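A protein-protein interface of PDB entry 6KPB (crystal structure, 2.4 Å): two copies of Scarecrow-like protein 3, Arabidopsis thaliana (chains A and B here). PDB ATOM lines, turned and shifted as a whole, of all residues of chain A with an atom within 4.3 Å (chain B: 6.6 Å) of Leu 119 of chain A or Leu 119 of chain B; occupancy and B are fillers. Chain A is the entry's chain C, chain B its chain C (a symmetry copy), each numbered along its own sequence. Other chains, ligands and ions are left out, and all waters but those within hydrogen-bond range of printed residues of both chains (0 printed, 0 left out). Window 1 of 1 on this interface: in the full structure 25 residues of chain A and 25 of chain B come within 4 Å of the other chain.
Along chain A the printed residues that touch a printed residue of chain B span positions 102 to 121. Of the 17 printed residues of chain B, 12 touch a printed residue of chain A. Printed residues of chain B that touch a printed residue of chain A: Leu 79, Ser 83, Thr 101, Glu 102, Ala 105, Ile 108, Leu 109, Leu 115, Ala 118, Leu 119, Ala 121 and Thr 122. Among the printed residues, 22 pairs touch across the chains.
Leu 119 of chain A touches just these residues of chain B: Glu 102 (3.7 Å), Ala 105 (3.6 Å), Leu 109 (3.6 Å) and Leu 119 (3.8 Å). Leu 119 of chain B touches four residues of chain A. Of the printed residues of chain A, Leu 79 of chain B touches Leu 115. Of the printed residues of chain A, Ser 83 of chain B touches Lys 117 and Ala 118. Of the printed residues of chain B, Leu 115 of chain A touches Leu 79, Ala 105 and Ile 108. Asn 120 of chain A touches none of the printed residues of chain B. Tyr 116 of chain A touches none of the printed residues of chain B. The nearest residue of chain B that does not touch Leu 119 of chain A is Asn 106 of chain B (4.4 Å).
The backbone carbonyl oxygen (O) of Leu 79 of chain B sits at hydrogen-bond distance from the side-chain hydroxyl (OG) of Ser 83 of chain B (3.0 Å).
Glu 102 of chain A touches Ala 121 of chain B, and with the chains exchanged Ala 121 of chain A touches Glu 102 of chain B. Ala 105 of chain A touches Leu 119 of chain B, and with the chains exchanged Leu 119 of chain A touches Ala 105 of chain B. Leu 109 of chain A touches Leu 119 of chain B, and with the chains exchanged Leu 119 of chain A touches Leu 109 of chain B. Leu 119 of chain B touches its own counterpart, Leu 119 of chain A. Of the 22 pairs that touch across the chains among the printed residues, 16 have their exchanged pair printed and touching as well.
The side-chain carboxylate of Glu 102 of chain A lies within hydrogen-bond range of the side-chain hydroxyl of Thr 122 of chain B (2.6 Å). The backbone NH (N) of Ala 118 of chain A is in hydrogen-bond range of the side-chain hydroxyl (OG) of Ser 83 of chain B (3.5 Å).
Among the printed residues, merely in contact across the chains: Glu 102 of chain A with Ala 118 of chain B (3.3 Å), Ala 118 of chain A with Glu 102 of chain B (3.3 Å), Lys 117 of chain A with Ser 83 of chain B (3.4 Å), Leu 115 of chain A with Ala 105 of chain B (3.5 Å), Ala 105 of chain A with Leu 115 of chain B (3.5 Å), Ala 118 of chain A with Thr 101 of chain B (3.6 Å), Leu 119 of chain A with Ala 105 of chain B (3.6 Å), Ala 105 of chain A with Leu 119 of chain B (3.6 Å), Ala 105 of chain A with Ala 118 of chain B (3.6 Å), Ala 118 of chain A with Ala 105 of chain B (3.6 Å), Leu 109 of chain A with Leu 119 of chain B (3.6 Å), Leu 119 of chain A with Leu 109 of chain B (3.6 Å), Leu 119 of chain A with Glu 102 of chain B (3.7 Å), Glu 102 of chain A with Leu 119 of chain B (3.7 Å), Leu 119 of chain A with Leu 119 of chain B (3.8 Å), Leu 115 of chain A with Ile 108 of chain B (3.9 Å), Leu 115 of chain A with Leu 79 of chain B (3.9 Å), Glu 102 of chain A with Ala 121 of chain B (3.96 Å), Ala 121 of chain A with Glu 102 of chain B (3.96 Å) and Leu 109 of chain A with Leu 109 of chain B (3.99 Å).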
ATOM      1  N   GLU A 102     -16.244 -13.224 -23.021  1.00  0.00           N
ATOM      2  CA  GLU A 102     -16.778 -11.875 -23.193  1.00  0.00           C
ATOM      3  C   GLU A 102     -17.932 -11.618 -22.234  1.00  0.00           C
ATOM      4  O   GLU A 102     -18.054 -10.522 -21.674  1.00  0.00           O
ATOM      5  CB  GLU A 102     -17.222 -11.664 -24.642  1.00  0.00           C
ATOM      6  CG  GLU A 102     -18.061 -10.411 -24.850  1.00  0.00           C
ATOM      7  CD  GLU A 102     -17.928  -9.830 -26.244  1.00  0.00           C
ATOM      8  OE1 GLU A 102     -17.105 -10.345 -27.029  1.00  0.00           O
ATOM      9  OE2 GLU A 102     -18.640  -8.852 -26.555  1.00  0.00           O
ATOM     10  N   ALA A 105     -16.484 -11.088 -18.710  1.00  0.00           N
ATOM     11  CA  ALA A 105     -15.851  -9.777 -18.636  1.00  0.00           C
ATOM     12  C   ALA A 105     -16.886  -8.661 -18.614  1.00  0.00           C
ATOM     13  O   ALA A 105     -16.664  -7.621 -17.984  1.00  0.00           O
ATOM     14  CB  ALA A 105     -14.886  -9.594 -19.805  1.00  0.00           C
ATOM     15  N   LEU A 109     -17.520  -5.934 -15.518  1.00  0.00           N
ATOM     16  CA  LEU A 109     -17.560  -4.531 -15.906  1.00  0.00           C
ATOM     17  C   LEU A 109     -18.749  -3.825 -15.272  1.00  0.00           C
ATOM     18  O   LEU A 109     -18.660  -2.637 -14.942  1.00  0.00           O
ATOM     19  CB  LEU A 109     -17.612  -4.409 -17.429  1.00  0.00           C
ATOM     20  CG  LEU A 109     -17.306  -3.031 -18.013  1.00  0.00           C
ATOM     21  CD1 LEU A 109     -15.905  -2.590 -17.621  1.00  0.00           C
ATOM     22  CD2 LEU A 109     -17.462  -3.043 -19.525  1.00  0.00           C
ATOM     23  N   LEU A 115     -17.686   3.261 -14.618  1.00  0.00           N
ATOM     24  CA  LEU A 115     -16.868   2.840 -15.750  1.00  0.00           C
ATOM     25  C   LEU A 115     -17.721   2.213 -16.846  1.00  0.00           C
ATOM     26  O   LEU A 115     -17.491   2.459 -18.036  1.00  0.00           O
ATOM     27  CB  LEU A 115     -15.792   1.861 -15.279  1.00  0.00           C
ATOM     28  CG  LEU A 115     -15.031   1.092 -16.360  1.00  0.00           C
ATOM     29  CD1 LEU A 115     -14.356   2.044 -17.338  1.00  0.00           C
ATOM     30  CD2 LEU A 115     -14.011   0.151 -15.735  1.00  0.00           C
ATOM     31  N   TYR A 116     -18.714   1.406 -16.465  1.00  0.00           N
ATOM     32  CA  TYR A 116     -19.557   0.745 -17.458  1.00  0.00           C
ATOM     33  C   TYR A 116     -20.352   1.761 -18.272  1.00  0.00           C
ATOM     34  O   TYR A 116     -20.402   1.684 -19.505  1.00  0.00           O
ATOM     35  CB  TYR A 116     -20.489  -0.253 -16.770  1.00  0.00           C
ATOM     36  CG  TYR A 116     -21.469  -0.923 -17.707  1.00  0.00           C
ATOM     37  CD1 TYR A 116     -21.097  -2.030 -18.459  1.00  0.00           C
ATOM     38  CD2 TYR A 116     -22.769  -0.449 -17.839  1.00  0.00           C
ATOM     39  CE1 TYR A 116     -21.991  -2.645 -19.316  1.00  0.00           C
ATOM     40  CE2 TYR A 116     -23.668  -1.057 -18.694  1.00  0.00           C
ATOM     41  CZ  TYR A 116     -23.275  -2.153 -19.429  1.00  0.00           C
ATOM     42  OH  TYR A 116     -24.169  -2.759 -20.279  1.00  0.00           O
ATOM     43  N   LYS A 117     -20.970   2.710 -17.613  1.00  0.00           N
ATOM     44  CA  LYS A 117     -21.742   3.727 -18.321  1.00  0.00           C
ATOM     45  C   LYS A 117     -20.845   4.597 -19.190  1.00  0.00           C
ATOM     46  O   LYS A 117     -21.175   4.883 -20.347  1.00  0.00           O
ATOM     47  CB  LYS A 117     -22.512   4.599 -17.330  1.00  0.00           C
ATOM     48  CG  LYS A 117     -23.585   3.881 -16.537  1.00  0.00           C
ATOM     49  CD  LYS A 117     -24.186   4.821 -15.505  1.00  0.00           C
ATOM     50  CE  LYS A 117     -24.880   4.058 -14.393  1.00  0.00           C
ATOM     51  NZ  LYS A 117     -25.406   4.983 -13.352  1.00  0.00           N
ATOM     52  N   ALA A 118     -19.725   5.046 -18.626  1.00  0.00           N
ATOM     53  CA  ALA A 118     -18.818   5.898 -19.385  1.00  0.00           C
ATOM     54  C   ALA A 118     -18.344   5.223 -20.668  1.00  0.00           C
ATOM     55  O   ALA A 118     -18.117   5.902 -21.675  1.00  0.00           O
ATOM     56  CB  ALA A 118     -17.627   6.294 -18.517  1.00  0.00           C
ATOM     57  N   LEU A 119     -18.203   3.894 -20.658  1.00  0.00           N
ATOM     58  CA  LEU A 119     -17.821   3.170 -21.867  1.00  0.00           C
ATOM     59  C   LEU A 119     -18.871   3.275 -22.965  1.00  0.00           C
ATOM     60  O   LEU A 119     -18.580   2.938 -24.120  1.00  0.00           O
ATOM     61  CB  LEU A 119     -17.565   1.693 -21.543  1.00  0.00           C
ATOM     62  CG  LEU A 119     -16.129   1.164 -21.584  1.00  0.00           C
ATOM     63  CD1 LEU A 119     -15.307   1.756 -20.460  1.00  0.00           C
ATOM     64  CD2 LEU A 119     -16.114  -0.355 -21.508  1.00  0.00           C
ATOM     65  N   ASN A 120     -20.083   3.722 -22.633  1.00  0.00           N
ATOM     66  CA  ASN A 120     -21.137   3.916 -23.622  1.00  0.00           C
ATOM     67  C   ASN A 120     -21.751   5.309 -23.530  1.00  0.00           C
ATOM     68  O   ASN A 120     -22.899   5.500 -23.945  1.00  0.00           O
ATOM     69  CB  ASN A 120     -22.222   2.849 -23.469  1.00  0.00           C
ATOM     70  CG  ASN A 120     -21.677   1.441 -23.596  1.00  0.00           C
ATOM     71  OD1 ASN A 120     -21.818   0.623 -22.686  1.00  0.00           O
ATOM     72  ND2 ASN A 120     -21.050   1.150 -24.730  1.00  0.00           N
ATOM     73  N   ALA A 121     -21.012   6.284 -22.990  1.00  0.00           N
ATOM     74  CA  ALA A 121     -21.537   7.643 -22.870  1.00  0.00           C
ATOM     75  C   ALA A 121     -21.956   8.193 -24.226  1.00  0.00           C
ATOM     76  O   ALA A 121     -22.961   8.904 -24.336  1.00  0.00           O
ATOM     77  CB  ALA A 121     -20.494   8.554 -22.223  1.00  0.00           C
ATOM     78  N   LEU B  79     -16.279   9.012 -12.980  1.00  0.00           N
ATOM     79  CA  LEU B  79     -16.937   8.625 -14.224  1.00  0.00           C
ATOM     80  C   LEU B  79     -18.445   8.514 -14.042  1.00  0.00           C
ATOM     81  O   LEU B  79     -19.211   8.822 -14.963  1.00  0.00           O
ATOM     82  CB  LEU B  79     -16.360   7.305 -14.737  1.00  0.00           C
ATOM     83  CG  LEU B  79     -14.922   7.340 -15.260  1.00  0.00           C
ATOM     84  CD1 LEU B  79     -14.479   5.958 -15.716  1.00  0.00           C
ATOM     85  CD2 LEU B  79     -14.787   8.352 -16.387  1.00  0.00           C
ATOM     86  N   SER B  83     -21.272  10.572 -16.378  1.00  0.00           N
ATOM     87  CA  SER B  83     -22.258   9.882 -17.207  1.00  0.00           C
ATOM     88  C   SER B  83     -23.611  10.580 -17.167  1.00  0.00           C
ATOM     89  O   SER B  83     -24.273  10.724 -18.202  1.00  0.00           O
ATOM     90  CB  SER B  83     -22.394   8.429 -16.758  1.00  0.00           C
ATOM     91  OG  SER B  83     -21.176   7.726 -16.933  1.00  0.00           O
ATOM     92  N   THR B 101     -15.078  11.624 -21.689  1.00  0.00           N
ATOM     93  CA  THR B 101     -15.397  10.642 -20.656  1.00  0.00           C
ATOM     94  C   THR B 101     -15.210   9.225 -21.179  1.00  0.00           C
ATOM     95  O   THR B 101     -14.568   8.391 -20.530  1.00  0.00           O
ATOM     96  CB  THR B 101     -16.827  10.842 -20.149  1.00  0.00           C
ATOM     97  OG1 THR B 101     -16.940  12.129 -19.525  1.00  0.00           O
ATOM     98  CG2 THR B 101     -17.197   9.768 -19.145  1.00  0.00           C
ATOM     99  N   GLU B 102     -15.771   8.933 -22.357  1.00  0.00           N
ATOM    100  CA  GLU B 102     -15.583   7.616 -22.957  1.00  0.00           C
ATOM    101  C   GLU B 102     -14.107   7.330 -23.198  1.00  0.00           C
ATOM    102  O   GLU B 102     -13.640   6.203 -22.989  1.00  0.00           O
ATOM    103  CB  GLU B 102     -16.373   7.513 -24.264  1.00  0.00           C
ATOM    104  CG  GLU B 102     -16.006   6.301 -25.110  1.00  0.00           C
ATOM    105  CD  GLU B 102     -17.151   5.810 -25.974  1.00  0.00           C
ATOM    106  OE1 GLU B 102     -18.268   6.351 -25.848  1.00  0.00           O
ATOM    107  OE2 GLU B 102     -16.936   4.876 -26.775  1.00  0.00           O
ATOM    108  N   ALA B 105     -12.462   6.527 -19.814  1.00  0.00           N
ATOM    109  CA  ALA B 105     -12.867   5.195 -19.380  1.00  0.00           C
ATOM    110  C   ALA B 105     -12.194   4.111 -20.210  1.00  0.00           C
ATOM    111  O   ALA B 105     -11.903   3.026 -19.695  1.00  0.00           O
ATOM    112  CB  ALA B 105     -14.386   5.061 -19.449  1.00  0.00           C
ATOM    113  N   ASN B 106     -11.931   4.386 -21.489  1.00  0.00           N
ATOM    114  CA  ASN B 106     -11.215   3.419 -22.314  1.00  0.00           C
ATOM    115  C   ASN B 106      -9.768   3.272 -21.858  1.00  0.00           C
ATOM    116  O   ASN B 106      -9.211   2.168 -21.891  1.00  0.00           O
ATOM    117  CB  ASN B 106     -11.275   3.834 -23.783  1.00  0.00           C
ATOM    118  CG  ASN B 106     -11.904   2.771 -24.667  1.00  0.00           C
ATOM    119  OD1 ASN B 106     -13.127   2.673 -24.767  1.00  0.00           O
ATOM    120  ND2 ASN B 106     -11.066   1.969 -25.315  1.00  0.00           N
ATOM    121  N   ILE B 108      -8.411   3.690 -18.736  1.00  0.00           N
ATOM    122  CA  ILE B 108      -8.318   2.888 -17.523  1.00  0.00           C
ATOM    123  C   ILE B 108      -8.735   1.451 -17.775  1.00  0.00           C
ATOM    124  O   ILE B 108      -8.334   0.551 -17.028  1.00  0.00           O
ATOM    125  CB  ILE B 108      -9.162   3.490 -16.387  1.00  0.00           C
ATOM    126  CG1 ILE B 108     -10.649   3.301 -16.664  1.00  0.00           C
ATOM    127  CG2 ILE B 108      -8.860   4.952 -16.230  1.00  0.00           C
ATOM    128  CD1 ILE B 108     -11.520   4.206 -15.837  1.00  0.00           C
ATOM    129  N   LEU B 109      -9.545   1.207 -18.807  1.00  0.00           N
ATOM    130  CA  LEU B 109      -9.848  -0.166 -19.187  1.00  0.00           C
ATOM    131  C   LEU B 109      -8.605  -0.878 -19.699  1.00  0.00           C
ATOM    132  O   LEU B 109      -8.453  -2.087 -19.492  1.00  0.00           O
ATOM    133  CB  LEU B 109     -10.952  -0.187 -20.244  1.00  0.00           C
ATOM    134  CG  LEU B 109     -11.632  -1.532 -20.495  1.00  0.00           C
ATOM    135  CD1 LEU B 109     -12.286  -2.039 -19.220  1.00  0.00           C
ATOM    136  CD2 LEU B 109     -12.654  -1.415 -21.614  1.00  0.00           C
ATOM    137  N   GLY B 114      -6.247  -8.180 -19.526  1.00  0.00           N
ATOM    138  CA  GLY B 114      -7.112  -9.346 -19.606  1.00  0.00           C
ATOM    139  C   GLY B 114      -8.573  -8.970 -19.755  1.00  0.00           C
ATOM    140  O   GLY B 114      -9.288  -9.517 -20.598  1.00  0.00           O
ATOM    141  N   LEU B 115      -9.035  -8.019 -18.939  1.00  0.00           N
ATOM    142  CA  LEU B 115     -10.411  -7.549 -19.053  1.00  0.00           C
ATOM    143  C   LEU B 115     -10.640  -6.827 -20.375  1.00  0.00           C
ATOM    144  O   LEU B 115     -11.687  -7.000 -21.009  1.00  0.00           O
ATOM    145  CB  LEU B 115     -10.748  -6.636 -17.874  1.00  0.00           C
ATOM    146  CG  LEU B 115     -12.038  -5.819 -17.974  1.00  0.00           C
ATOM    147  CD1 LEU B 115     -13.244  -6.724 -18.183  1.00  0.00           C
ATOM    148  CD2 LEU B 115     -12.223  -4.952 -16.737  1.00  0.00           C
ATOM    149  N   TYR B 116      -9.671  -6.017 -20.808  1.00  0.00           N
ATOM    150  CA  TYR B 116      -9.830  -5.268 -22.052  1.00  0.00           C
ATOM    151  C   TYR B 116      -9.936  -6.204 -23.252  1.00  0.00           C
ATOM    152  O   TYR B 116     -10.820  -6.045 -24.102  1.00  0.00           O
ATOM    153  CB  TYR B 116      -8.667  -4.290 -22.225  1.00  0.00           C
ATOM    154  CG  TYR B 116      -8.692  -3.531 -23.532  1.00  0.00           C
ATOM    155  CD1 TYR B 116      -9.468  -2.388 -23.681  1.00  0.00           C
ATOM    156  CD2 TYR B 116      -7.939  -3.957 -24.620  1.00  0.00           C
ATOM    157  CE1 TYR B 116      -9.493  -1.692 -24.876  1.00  0.00           C
ATOM    158  CE2 TYR B 116      -7.958  -3.268 -25.817  1.00  0.00           C
ATOM    159  CZ  TYR B 116      -8.736  -2.138 -25.940  1.00  0.00           C
ATOM    160  OH  TYR B 116      -8.756  -1.451 -27.131  1.00  0.00           O
ATOM    161  N   LYS B 117      -9.062  -7.176 -23.337  1.00  0.00           N
ATOM    162  CA  LYS B 117      -9.105  -8.121 -24.450  1.00  0.00           C
ATOM    163  C   LYS B 117     -10.376  -8.958 -24.415  1.00  0.00           C
ATOM    164  O   LYS B 117     -11.027  -9.157 -25.448  1.00  0.00           O
ATOM    165  CB  LYS B 117      -7.879  -9.033 -24.423  1.00  0.00           C
ATOM    166  CG  LYS B 117      -6.552  -8.337 -24.649  1.00  0.00           C
ATOM    167  CD  LYS B 117      -5.411  -9.325 -24.473  1.00  0.00           C
ATOM    168  CE  LYS B 117      -4.097  -8.616 -24.202  1.00  0.00           C
ATOM    169  NZ  LYS B 117      -2.999  -9.592 -23.965  1.00  0.00           N
ATOM    170  N   ALA B 118     -10.715  -9.476 -23.236  1.00  0.00           N
ATOM    171  CA  ALA B 118     -11.910 -10.303 -23.120  1.00  0.00           C
ATOM    172  C   ALA B 118     -13.162  -9.558 -23.574  1.00  0.00           C
ATOM    173  O   ALA B 118     -14.084 -10.176 -24.117  1.00  0.00           O
ATOM    174  CB  ALA B 118     -12.069 -10.789 -21.682  1.00  0.00           C
ATOM    175  N   LEU B 119     -13.210  -8.237 -23.375  1.00  0.00           N
ATOM    176  CA  LEU B 119     -14.343  -7.447 -23.844  1.00  0.00           C
ATOM    177  C   LEU B 119     -14.465  -7.449 -25.362  1.00  0.00           C
ATOM    178  O   LEU B 119     -15.509  -7.045 -25.891  1.00  0.00           O
ATOM    179  CB  LEU B 119     -14.229  -6.003 -23.342  1.00  0.00           C
ATOM    180  CG  LEU B 119     -15.201  -5.515 -22.264  1.00  0.00           C
ATOM    181  CD1 LEU B 119     -14.928  -6.204 -20.945  1.00  0.00           C
ATOM    182  CD2 LEU B 119     -15.109  -4.005 -22.102  1.00  0.00           C
ATOM    183  N   ASN B 120     -13.423  -7.881 -26.075  1.00  0.00           N
ATOM    184  CA  ASN B 120     -13.464  -7.979 -27.529  1.00  0.00           C
ATOM    185  C   ASN B 120     -13.027  -9.356 -28.017  1.00  0.00           C
ATOM    186  O   ASN B 120     -12.577  -9.485 -29.161  1.00  0.00           O
ATOM    187  CB  ASN B 120     -12.595  -6.892 -28.166  1.00  0.00           C
ATOM    188  CG  ASN B 120     -13.012  -5.496 -27.752  1.00  0.00           C
ATOM    189  OD1 ASN B 120     -12.216  -4.735 -27.199  1.00  0.00           O
ATOM    190  ND2 ASN B 120     -14.266  -5.149 -28.017  1.00  0.00           N
ATOM    191  N   ALA B 121     -13.146 -10.386 -27.173  1.00  0.00           N
ATOM    192  CA  ALA B 121     -12.747 -11.733 -27.573  1.00  0.00           C
ATOM    193  C   ALA B 121     -13.494 -12.180 -28.822  1.00  0.00           C
ATOM    194  O   ALA B 121     -12.927 -12.853 -29.690  1.00  0.00           O
ATOM    195  CB  ALA B 121     -12.987 -12.715 -26.427  1.00  0.00           C
ATOM    196  N   THR B 122     -14.767 -11.812 -28.929  1.00  0.00           N
ATOM    197  CA  THR B 122     -15.554 -12.072 -30.131  1.00  0.00           C
ATOM    198  C   THR B 122     -15.415 -10.900 -31.101  1.00  0.00           C
ATOM    199  O   THR B 122     -16.373 -10.191 -31.412  1.00  0.00           O
ATOM    200  CB  THR B 122     -17.010 -12.316 -29.759  1.00  0.00           C
ATOM    201  OG1 THR B 122     -17.650 -11.059 -29.504  1.00  0.00           O
ATOM    202  CG2 THR B 122     -17.081 -13.163 -28.505  1.00  0.00           C
